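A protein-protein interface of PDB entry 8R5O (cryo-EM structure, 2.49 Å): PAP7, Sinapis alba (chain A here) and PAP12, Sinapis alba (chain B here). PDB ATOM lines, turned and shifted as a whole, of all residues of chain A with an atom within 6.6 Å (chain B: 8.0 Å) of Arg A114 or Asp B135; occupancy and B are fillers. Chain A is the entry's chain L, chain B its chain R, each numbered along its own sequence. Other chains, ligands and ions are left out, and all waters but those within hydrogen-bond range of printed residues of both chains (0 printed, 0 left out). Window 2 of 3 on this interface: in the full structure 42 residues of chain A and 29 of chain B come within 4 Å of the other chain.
O of Asn B134 lies within hydrogen-bond range of NH1 of Arg A113 (2.5 Å). NH1 of Arg A114 is in salt-bridge range of OE2 of Glu B106. The side-chain carboxylate (OD2) of Asp B135 is in salt-bridge range of the guanidinium group (NE) of Arg A114 (3.8 Å). The guanidinium group (NH2) of Arg A117 lies within hydrogen-bond range of the backbone carbonyl oxygen (O) of Gly B137 (3.1 Å). O of Leu B136 is in hydrogen-bond range of N of Val A118, 3.0 Å away.
Among the printed residues, merely in contact across the chains: Arg A113 with Asp B135, Arg A113 with Gly B137, Arg A113 with Phe B138, Arg A114 with Tyr B110, Arg A115 with Asp B135, Ala A116 with Asp B135, Arg A117 with Asp B135 and Arg A117 with Leu B136.
Printed residues of chain B that touch a printed residue of chain A: Glu B106, Tyr B110, Asn B134, Asp B135, Leu B136, Gly B137 and Phe B138. Hydrophobic or aromatic side chains of chain B within 4 Å of the printed part of chain A: Tyr B110. Hydrophobic or aromatic side chains of chain A within 4 Å of the printed part of chain B: Val A118.
N of Gly A311 is in hydrogen-bond range of O of Arg A113, 3.2 Å away. The side-chain hydroxyl of Tyr B110 sits at hydrogen-bond distance from the side-chain carboxylate of Glu B106 (2.8 Å). The side-chain carboxylate of Glu B106 is in salt-bridge range of the guanidinium group of Arg B132, at 2.8 Å. The side-chain amide nitrogen (ND2) of Asn B131 lies within hydrogen-bond range of the side-chain hydroxyl (OH) of Tyr B110, 2.8 Å away. O of Ser B130 lies within hydrogen-bond range of ND2 of Asn B134, at 3.1 Å. The backbone carbonyl oxygen (O) of Phe B138 lies close to the side-chain amide oxygen (OD1) of Asn B134 (2.8 Å).
Arg A114 touches just these residues of chain B: Glu B106, Tyr B110 and Asp B135. Printed residues of chain B within 4 Å of Arg A115: Asp B135. Val B128 touches none of the printed residues of chain A. Printed residues of chain A within 4 Å of Asp B135: Arg A113, Arg A114, Arg A115, Ala A116 and Arg A117. Of the printed residues of chain A, Gly B137 touches Arg A113 and Arg A117. Asp B139 touches none of the printed residues of chain A. The nearest printed residue of chain A that does not touch Tyr B110 is Arg A115 (10.4 Å).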
ATOM      1  N   PRO A 112      13.275 -26.561  38.174  1.00  0.00           N
ATOM      2  CA  PRO A 112      14.464 -27.359  37.863  1.00  0.00           C
ATOM      3  C   PRO A 112      14.852 -27.246  36.397  1.00  0.00           C
ATOM      4  O   PRO A 112      14.012 -27.047  35.517  1.00  0.00           O
ATOM      5  CB  PRO A 112      14.033 -28.786  38.214  1.00  0.00           C
ATOM      6  CG  PRO A 112      12.556 -28.774  38.050  1.00  0.00           C
ATOM      7  CD  PRO A 112      12.105 -27.404  38.471  1.00  0.00           C
ATOM      8  N   ARG A 113      16.152 -27.376  36.146  1.00  0.00           N
ATOM      9  CA  ARG A 113      16.714 -27.351  34.805  1.00  0.00           C
ATOM     10  C   ARG A 113      17.639 -28.550  34.635  1.00  0.00           C
ATOM     11  O   ARG A 113      17.861 -29.330  35.565  1.00  0.00           O
ATOM     12  CB  ARG A 113      17.459 -26.036  34.542  1.00  0.00           C
ATOM     13  CG  ARG A 113      16.565 -24.811  34.538  1.00  0.00           C
ATOM     14  CD  ARG A 113      15.652 -24.805  33.325  1.00  0.00           C
ATOM     15  NE  ARG A 113      14.473 -23.973  33.530  1.00  0.00           N
ATOM     16  CZ  ARG A 113      14.448 -22.655  33.392  1.00  0.00           C
ATOM     17  NH1 ARG A 113      15.534 -21.973  33.063  1.00  0.00           N
ATOM     18  NH2 ARG A 113      13.308 -22.002  33.596  1.00  0.00           N
ATOM     19  N   ARG A 114      18.181 -28.699  33.425  1.00  0.00           N
ATOM     20  CA  ARG A 114      19.119 -29.785  33.165  1.00  0.00           C
ATOM     21  C   ARG A 114      20.438 -29.577  33.895  1.00  0.00           C
ATOM     22  O   ARG A 114      21.133 -30.549  34.206  1.00  0.00           O
ATOM     23  CB  ARG A 114      19.370 -29.916  31.664  1.00  0.00           C
ATOM     24  CG  ARG A 114      18.134 -30.223  30.846  1.00  0.00           C
ATOM     25  CD  ARG A 114      18.399 -29.982  29.372  1.00  0.00           C
ATOM     26  NE  ARG A 114      19.607 -30.661  28.922  1.00  0.00           N
ATOM     27  CZ  ARG A 114      20.158 -30.494  27.727  1.00  0.00           C
ATOM     28  NH1 ARG A 114      19.635 -29.670  26.835  1.00  0.00           N
ATOM     29  NH2 ARG A 114      21.262 -31.171  27.422  1.00  0.00           N
ATOM     30  N   ARG A 115      20.797 -28.329  34.176  1.00  0.00           N
ATOM     31  CA  ARG A 115      22.053 -28.003  34.829  1.00  0.00           C
ATOM     32  C   ARG A 115      21.785 -27.119  36.038  1.00  0.00           C
ATOM     33  O   ARG A 115      20.664 -26.661  36.268  1.00  0.00           O
ATOM     34  CB  ARG A 115      23.021 -27.302  33.866  1.00  0.00           C
ATOM     35  CG  ARG A 115      23.554 -28.183  32.743  1.00  0.00           C
ATOM     36  CD  ARG A 115      24.399 -29.336  33.272  1.00  0.00           C
ATOM     37  NE  ARG A 115      25.167 -28.965  34.456  1.00  0.00           N
ATOM     38  CZ  ARG A 115      25.027 -29.534  35.647  1.00  0.00           C
ATOM     39  NH1 ARG A 115      24.192 -30.544  35.835  1.00  0.00           N
ATOM     40  NH2 ARG A 115      25.745 -29.083  36.670  1.00  0.00           N
ATOM     41  N   ALA A 116      22.838 -26.891  36.818  1.00  0.00           N
ATOM     42  CA  ALA A 116      22.738 -26.015  37.975  1.00  0.00           C
ATOM     43  C   ALA A 116      22.419 -24.590  37.542  1.00  0.00           C
ATOM     44  O   ALA A 116      22.995 -24.070  36.583  1.00  0.00           O
ATOM     45  CB  ALA A 116      24.041 -26.045  38.774  1.00  0.00           C
ATOM     46  N   ARG A 117      21.493 -23.958  38.255  1.00  0.00           N
ATOM     47  CA  ARG A 117      21.104 -22.587  37.967  1.00  0.00           C
ATOM     48  C   ARG A 117      21.967 -21.621  38.765  1.00  0.00           C
ATOM     49  O   ARG A 117      22.317 -21.889  39.915  1.00  0.00           O
ATOM     50  CB  ARG A 117      19.631 -22.359  38.300  1.00  0.00           C
ATOM     51  CG  ARG A 117      18.667 -23.209  37.497  1.00  0.00           C
ATOM     52  CD  ARG A 117      17.246 -23.003  37.981  1.00  0.00           C
ATOM     53  NE  ARG A 117      16.794 -21.631  37.780  1.00  0.00           N
ATOM     54  CZ  ARG A 117      15.764 -21.287  37.020  1.00  0.00           C
ATOM     55  NH1 ARG A 117      15.026 -22.194  36.404  1.00  0.00           N
ATOM     56  NH2 ARG A 117      15.463 -19.999  36.880  1.00  0.00           N
ATOM     57  N   VAL A 118      22.302 -20.495  38.147  1.00  0.00           N
ATOM     58  CA  VAL A 118      23.063 -19.452  38.825  1.00  0.00           C
ATOM     59  C   VAL A 118      22.122 -18.695  39.751  1.00  0.00           C
ATOM     60  O   VAL A 118      21.122 -18.123  39.307  1.00  0.00           O
ATOM     61  CB  VAL A 118      23.728 -18.505  37.817  1.00  0.00           C
ATOM     62  CG1 VAL A 118      24.599 -17.496  38.541  1.00  0.00           C
ATOM     63  CG2 VAL A 118      24.542 -19.293  36.803  1.00  0.00           C
ATOM     64  N   ALA A 310      21.468 -29.067  40.402  1.00  0.00           N
ATOM     65  CA  ALA A 310      20.873 -29.351  39.104  1.00  0.00           C
ATOM     66  C   ALA A 310      19.696 -30.306  39.249  1.00  0.00           C
ATOM     67  O   ALA A 310      19.797 -31.343  39.910  1.00  0.00           O
ATOM     68  CB  ALA A 310      21.919 -29.942  38.162  1.00  0.00           C
ATOM     69  N   GLY A 311      18.574 -29.949  38.628  1.00  0.00           N
ATOM     70  CA  GLY A 311      17.388 -30.772  38.661  1.00  0.00           C
ATOM     71  C   GLY A 311      16.543 -30.640  39.907  1.00  0.00           C
ATOM     72  O   GLY A 311      15.513 -31.319  40.009  1.00  0.00           O
ATOM     73  N   LEU B  89      28.476 -18.123  27.971  1.00  0.00           N
ATOM     74  CA  LEU B  89      28.735 -19.552  28.106  1.00  0.00           C
ATOM     75  C   LEU B  89      30.226 -19.857  28.144  1.00  0.00           C
ATOM     76  O   LEU B  89      30.649 -20.773  28.855  1.00  0.00           O
ATOM     77  CB  LEU B  89      28.065 -20.319  26.967  1.00  0.00           C
ATOM     78  CG  LEU B  89      26.538 -20.290  26.942  1.00  0.00           C
ATOM     79  CD1 LEU B  89      26.006 -21.020  25.723  1.00  0.00           C
ATOM     80  CD2 LEU B  89      25.973 -20.892  28.215  1.00  0.00           C
ATOM     81  N   GLU B 106      25.849 -32.075  20.703  1.00  0.00           N
ATOM     82  CA  GLU B 106      24.461 -31.921  21.126  1.00  0.00           C
ATOM     83  C   GLU B 106      23.556 -31.559  19.956  1.00  0.00           C
ATOM     84  O   GLU B 106      22.401 -31.995  19.910  1.00  0.00           O
ATOM     85  CB  GLU B 106      24.362 -30.868  22.228  1.00  0.00           C
ATOM     86  CG  GLU B 106      22.978 -30.732  22.839  1.00  0.00           C
ATOM     87  CD  GLU B 106      22.960 -29.823  24.051  1.00  0.00           C
ATOM     88  OE1 GLU B 106      24.022 -29.645  24.682  1.00  0.00           O
ATOM     89  OE2 GLU B 106      21.881 -29.282  24.372  1.00  0.00           O
ATOM     90  N   TYR B 110      20.041 -33.524  18.302  1.00  0.00           N
ATOM     91  CA  TYR B 110      18.744 -32.919  18.013  1.00  0.00           C
ATOM     92  C   TYR B 110      18.228 -33.343  16.643  1.00  0.00           C
ATOM     93  O   TYR B 110      17.043 -33.656  16.488  1.00  0.00           O
ATOM     94  CB  TYR B 110      18.832 -31.393  18.078  1.00  0.00           C
ATOM     95  CG  TYR B 110      18.980 -30.795  19.462  1.00  0.00           C
ATOM     96  CD1 TYR B 110      19.189 -31.595  20.577  1.00  0.00           C
ATOM     97  CD2 TYR B 110      18.898 -29.422  19.650  1.00  0.00           C
ATOM     98  CE1 TYR B 110      19.325 -31.041  21.837  1.00  0.00           C
ATOM     99  CE2 TYR B 110      19.028 -28.861  20.904  1.00  0.00           C
ATOM    100  CZ  TYR B 110      19.243 -29.675  21.994  1.00  0.00           C
ATOM    101  OH  TYR B 110      19.374 -29.117  23.244  1.00  0.00           O
ATOM    102  N   LYS B 113      17.013 -36.930  16.557  1.00  0.00           N
ATOM    103  CA  LYS B 113      15.768 -37.085  17.301  1.00  0.00           C
ATOM    104  C   LYS B 113      14.581 -36.543  16.513  1.00  0.00           C
ATOM    105  O   LYS B 113      13.564 -37.228  16.355  1.00  0.00           O
ATOM    106  CB  LYS B 113      15.886 -36.378  18.653  1.00  0.00           C
ATOM    107  CG  LYS B 113      14.951 -36.896  19.731  1.00  0.00           C
ATOM    108  CD  LYS B 113      14.631 -35.807  20.745  1.00  0.00           C
ATOM    109  CE  LYS B 113      15.869 -35.007  21.121  1.00  0.00           C
ATOM    110  NZ  LYS B 113      15.517 -33.768  21.867  1.00  0.00           N
ATOM    111  N   HIS B 127      19.347 -23.683  18.595  1.00  0.00           N
ATOM    112  CA  HIS B 127      18.555 -24.314  19.643  1.00  0.00           C
ATOM    113  C   HIS B 127      19.432 -24.767  20.804  1.00  0.00           C
ATOM    114  O   HIS B 127      19.043 -24.642  21.971  1.00  0.00           O
ATOM    115  CB  HIS B 127      17.775 -25.493  19.063  1.00  0.00           C
ATOM    116  CG  HIS B 127      16.684 -25.996  19.956  1.00  0.00           C
ATOM    117  ND1 HIS B 127      16.037 -27.193  19.737  1.00  0.00           N
ATOM    118  CD2 HIS B 127      16.122 -25.461  21.065  1.00  0.00           C
ATOM    119  CE1 HIS B 127      15.126 -27.376  20.676  1.00  0.00           C
ATOM    120  NE2 HIS B 127      15.157 -26.339  21.493  1.00  0.00           N
ATOM    121  N   VAL B 128      20.615 -25.305  20.503  1.00  0.00           N
ATOM    122  CA  VAL B 128      21.524 -25.756  21.555  1.00  0.00           C
ATOM    123  C   VAL B 128      21.956 -24.583  22.424  1.00  0.00           C
ATOM    124  O   VAL B 128      21.953 -24.666  23.657  1.00  0.00           O
ATOM    125  CB  VAL B 128      22.739 -26.478  20.942  1.00  0.00           C
ATOM    126  CG1 VAL B 128      23.805 -26.720  21.997  1.00  0.00           C
ATOM    127  CG2 VAL B 128      22.314 -27.785  20.300  1.00  0.00           C
ATOM    128  N   LEU B 129      22.329 -23.467  21.792  1.00  0.00           N
ATOM    129  CA  LEU B 129      22.817 -22.317  22.544  1.00  0.00           C
ATOM    130  C   LEU B 129      21.729 -21.722  23.430  1.00  0.00           C
ATOM    131  O   LEU B 129      21.993 -21.354  24.579  1.00  0.00           O
ATOM    132  CB  LEU B 129      23.370 -21.261  21.590  1.00  0.00           C
ATOM    133  CG  LEU B 129      24.627 -21.657  20.816  1.00  0.00           C
ATOM    134  CD1 LEU B 129      25.130 -20.493  19.983  1.00  0.00           C
ATOM    135  CD2 LEU B 129      25.706 -22.148  21.766  1.00  0.00           C
ATOM    136  N   SER B 130      20.503 -21.617  22.915  1.00  0.00           N
ATOM    137  CA  SER B 130      19.411 -21.091  23.727  1.00  0.00           C
ATOM    138  C   SER B 130      19.053 -22.034  24.867  1.00  0.00           C
ATOM    139  O   SER B 130      18.709 -21.575  25.961  1.00  0.00           O
ATOM    140  CB  SER B 130      18.183 -20.819  22.855  1.00  0.00           C
ATOM    141  OG  SER B 130      17.668 -22.018  22.308  1.00  0.00           O
ATOM    142  N   ASN B 131      19.125 -23.347  24.634  1.00  0.00           N
ATOM    143  CA  ASN B 131      18.876 -24.303  25.708  1.00  0.00           C
ATOM    144  C   ASN B 131      19.913 -24.179  26.814  1.00  0.00           C
ATOM    145  O   ASN B 131      19.579 -24.270  27.999  1.00  0.00           O
ATOM    146  CB  ASN B 131      18.857 -25.727  25.158  1.00  0.00           C
ATOM    147  CG  ASN B 131      17.553 -26.071  24.481  1.00  0.00           C
ATOM    148  OD1 ASN B 131      16.708 -25.204  24.263  1.00  0.00           O
ATOM    149  ND2 ASN B 131      17.380 -27.341  24.143  1.00  0.00           N
ATOM    150  N   ARG B 132      21.180 -23.979  26.448  1.00  0.00           N
ATOM    151  CA  ARG B 132      22.226 -23.901  27.460  1.00  0.00           C
ATOM    152  C   ARG B 132      22.153 -22.604  28.251  1.00  0.00           C
ATOM    153  O   ARG B 132      22.578 -22.563  29.410  1.00  0.00           O
ATOM    154  CB  ARG B 132      23.599 -24.059  26.812  1.00  0.00           C
ATOM    155  CG  ARG B 132      23.811 -25.424  26.198  1.00  0.00           C
ATOM    156  CD  ARG B 132      25.272 -25.706  25.954  1.00  0.00           C
ATOM    157  NE  ARG B 132      25.466 -27.037  25.395  1.00  0.00           N
ATOM    158  CZ  ARG B 132      26.641 -27.643  25.295  1.00  0.00           C
ATOM    159  NH1 ARG B 132      27.750 -27.073  25.734  1.00  0.00           N
ATOM    160  NH2 ARG B 132      26.702 -28.849  24.742  1.00  0.00           N
ATOM    161  N   VAL B 133      21.633 -21.535  27.647  1.00  0.00           N
ATOM    162  CA  VAL B 133      21.383 -20.316  28.406  1.00  0.00           C
ATOM    163  C   VAL B 133      20.216 -20.519  29.364  1.00  0.00           C
ATOM    164  O   VAL B 133      20.256 -20.074  30.518  1.00  0.00           O
ATOM    165  CB  VAL B 133      21.144 -19.129  27.455  1.00  0.00           C
ATOM    166  CG1 VAL B 133      20.807 -17.877  28.243  1.00  0.00           C
ATOM    167  CG2 VAL B 133      22.369 -18.896  26.590  1.00  0.00           C
ATOM    168  N   ASN B 134      19.163 -21.201  28.907  1.00  0.00           N
ATOM    169  CA  ASN B 134      18.030 -21.486  29.781  1.00  0.00           C
ATOM    170  C   ASN B 134      18.404 -22.452  30.897  1.00  0.00           C
ATOM    171  O   ASN B 134      17.786 -22.426  31.967  1.00  0.00           O
ATOM    172  CB  ASN B 134      16.861 -22.045  28.968  1.00  0.00           C
ATOM    173  CG  ASN B 134      16.265 -21.020  28.021  1.00  0.00           C
ATOM    174  OD1 ASN B 134      16.263 -19.824  28.301  1.00  0.00           O
ATOM    175  ND2 ASN B 134      15.750 -21.491  26.892  1.00  0.00           N
ATOM    176  N   ASP B 135      19.402 -23.310  30.671  1.00  0.00           N
ATOM    177  CA  ASP B 135      19.838 -24.224  31.721  1.00  0.00           C
ATOM    178  C   ASP B 135      20.497 -23.481  32.874  1.00  0.00           C
ATOM    179  O   ASP B 135      20.451 -23.947  34.017  1.00  0.00           O
ATOM    180  CB  ASP B 135      20.793 -25.270  31.147  1.00  0.00           C
ATOM    181  CG  ASP B 135      20.097 -26.253  30.228  1.00  0.00           C
ATOM    182  OD1 ASP B 135      18.860 -26.157  30.081  1.00  0.00           O
ATOM    183  OD2 ASP B 135      20.786 -27.120  29.651  1.00  0.00           O
ATOM    184  N   LEU B 136      21.115 -22.332  32.597  1.00  0.00           N
ATOM    185  CA  LEU B 136      21.671 -21.494  33.652  1.00  0.00           C
ATOM    186  C   LEU B 136      20.596 -20.796  34.474  1.00  0.00           C
ATOM    187  O   LEU B 136      20.922 -20.192  35.500  1.00  0.00           O
ATOM    188  CB  LEU B 136      22.617 -20.455  33.050  1.00  0.00           C
ATOM    189  CG  LEU B 136      23.898 -20.996  32.416  1.00  0.00           C
ATOM    190  CD1 LEU B 136      24.714 -19.868  31.809  1.00  0.00           C
ATOM    191  CD2 LEU B 136      24.713 -21.751  33.448  1.00  0.00           C
ATOM    192  N   GLY B 137      19.336 -20.866  34.054  1.00  0.00           N
ATOM    193  CA  GLY B 137      18.246 -20.214  34.744  1.00  0.00           C
ATOM    194  C   GLY B 137      17.766 -18.925  34.116  1.00  0.00           C
ATOM    195  O   GLY B 137      16.817 -18.323  34.632  1.00  0.00           O
ATOM    196  N   PHE B 138      18.383 -18.484  33.027  1.00  0.00           N
ATOM    197  CA  PHE B 138      17.945 -17.288  32.330  1.00  0.00           C
ATOM    198  C   PHE B 138      16.937 -17.656  31.243  1.00  0.00           C
ATOM    199  O   PHE B 138      16.729 -18.827  30.925  1.00  0.00           O
ATOM    200  CB  PHE B 138      19.146 -16.546  31.749  1.00  0.00           C
ATOM    201  CG  PHE B 138      20.238 -16.300  32.749  1.00  0.00           C
ATOM    202  CD1 PHE B 138      20.068 -15.375  33.766  1.00  0.00           C
ATOM    203  CD2 PHE B 138      21.430 -16.998  32.678  1.00  0.00           C
ATOM    204  CE1 PHE B 138      21.068 -15.151  34.689  1.00  0.00           C
ATOM    205  CE2 PHE B 138      22.434 -16.778  33.598  1.00  0.00           C
ATOM    206  CZ  PHE B 138      22.253 -15.854  34.606  1.00  0.00           C
ATOM    207  N   ASP B 139      16.294 -16.638  30.679  1.00  0.00           N
ATOM    208  CA  ASP B 139      15.215 -16.834  29.720  1.00  0.00           C
ATOM    209  C   ASP B 139      15.610 -16.287  28.358  1.00  0.00           C
ATOM    210  O   ASP B 139      16.022 -15.129  28.243  1.00  0.00           O
ATOM    211  CB  ASP B 139      13.925 -16.165  30.200  1.00  0.00           C
ATOM    212  CG  ASP B 139      13.218 -16.972  31.267  1.00  0.00           C
ATOM    213  OD1 ASP B 139      13.726 -17.034  32.406  1.00  0.00           O
ATOM    214  OD2 ASP B 139      12.156 -17.552  30.961  1.00  0.00           O
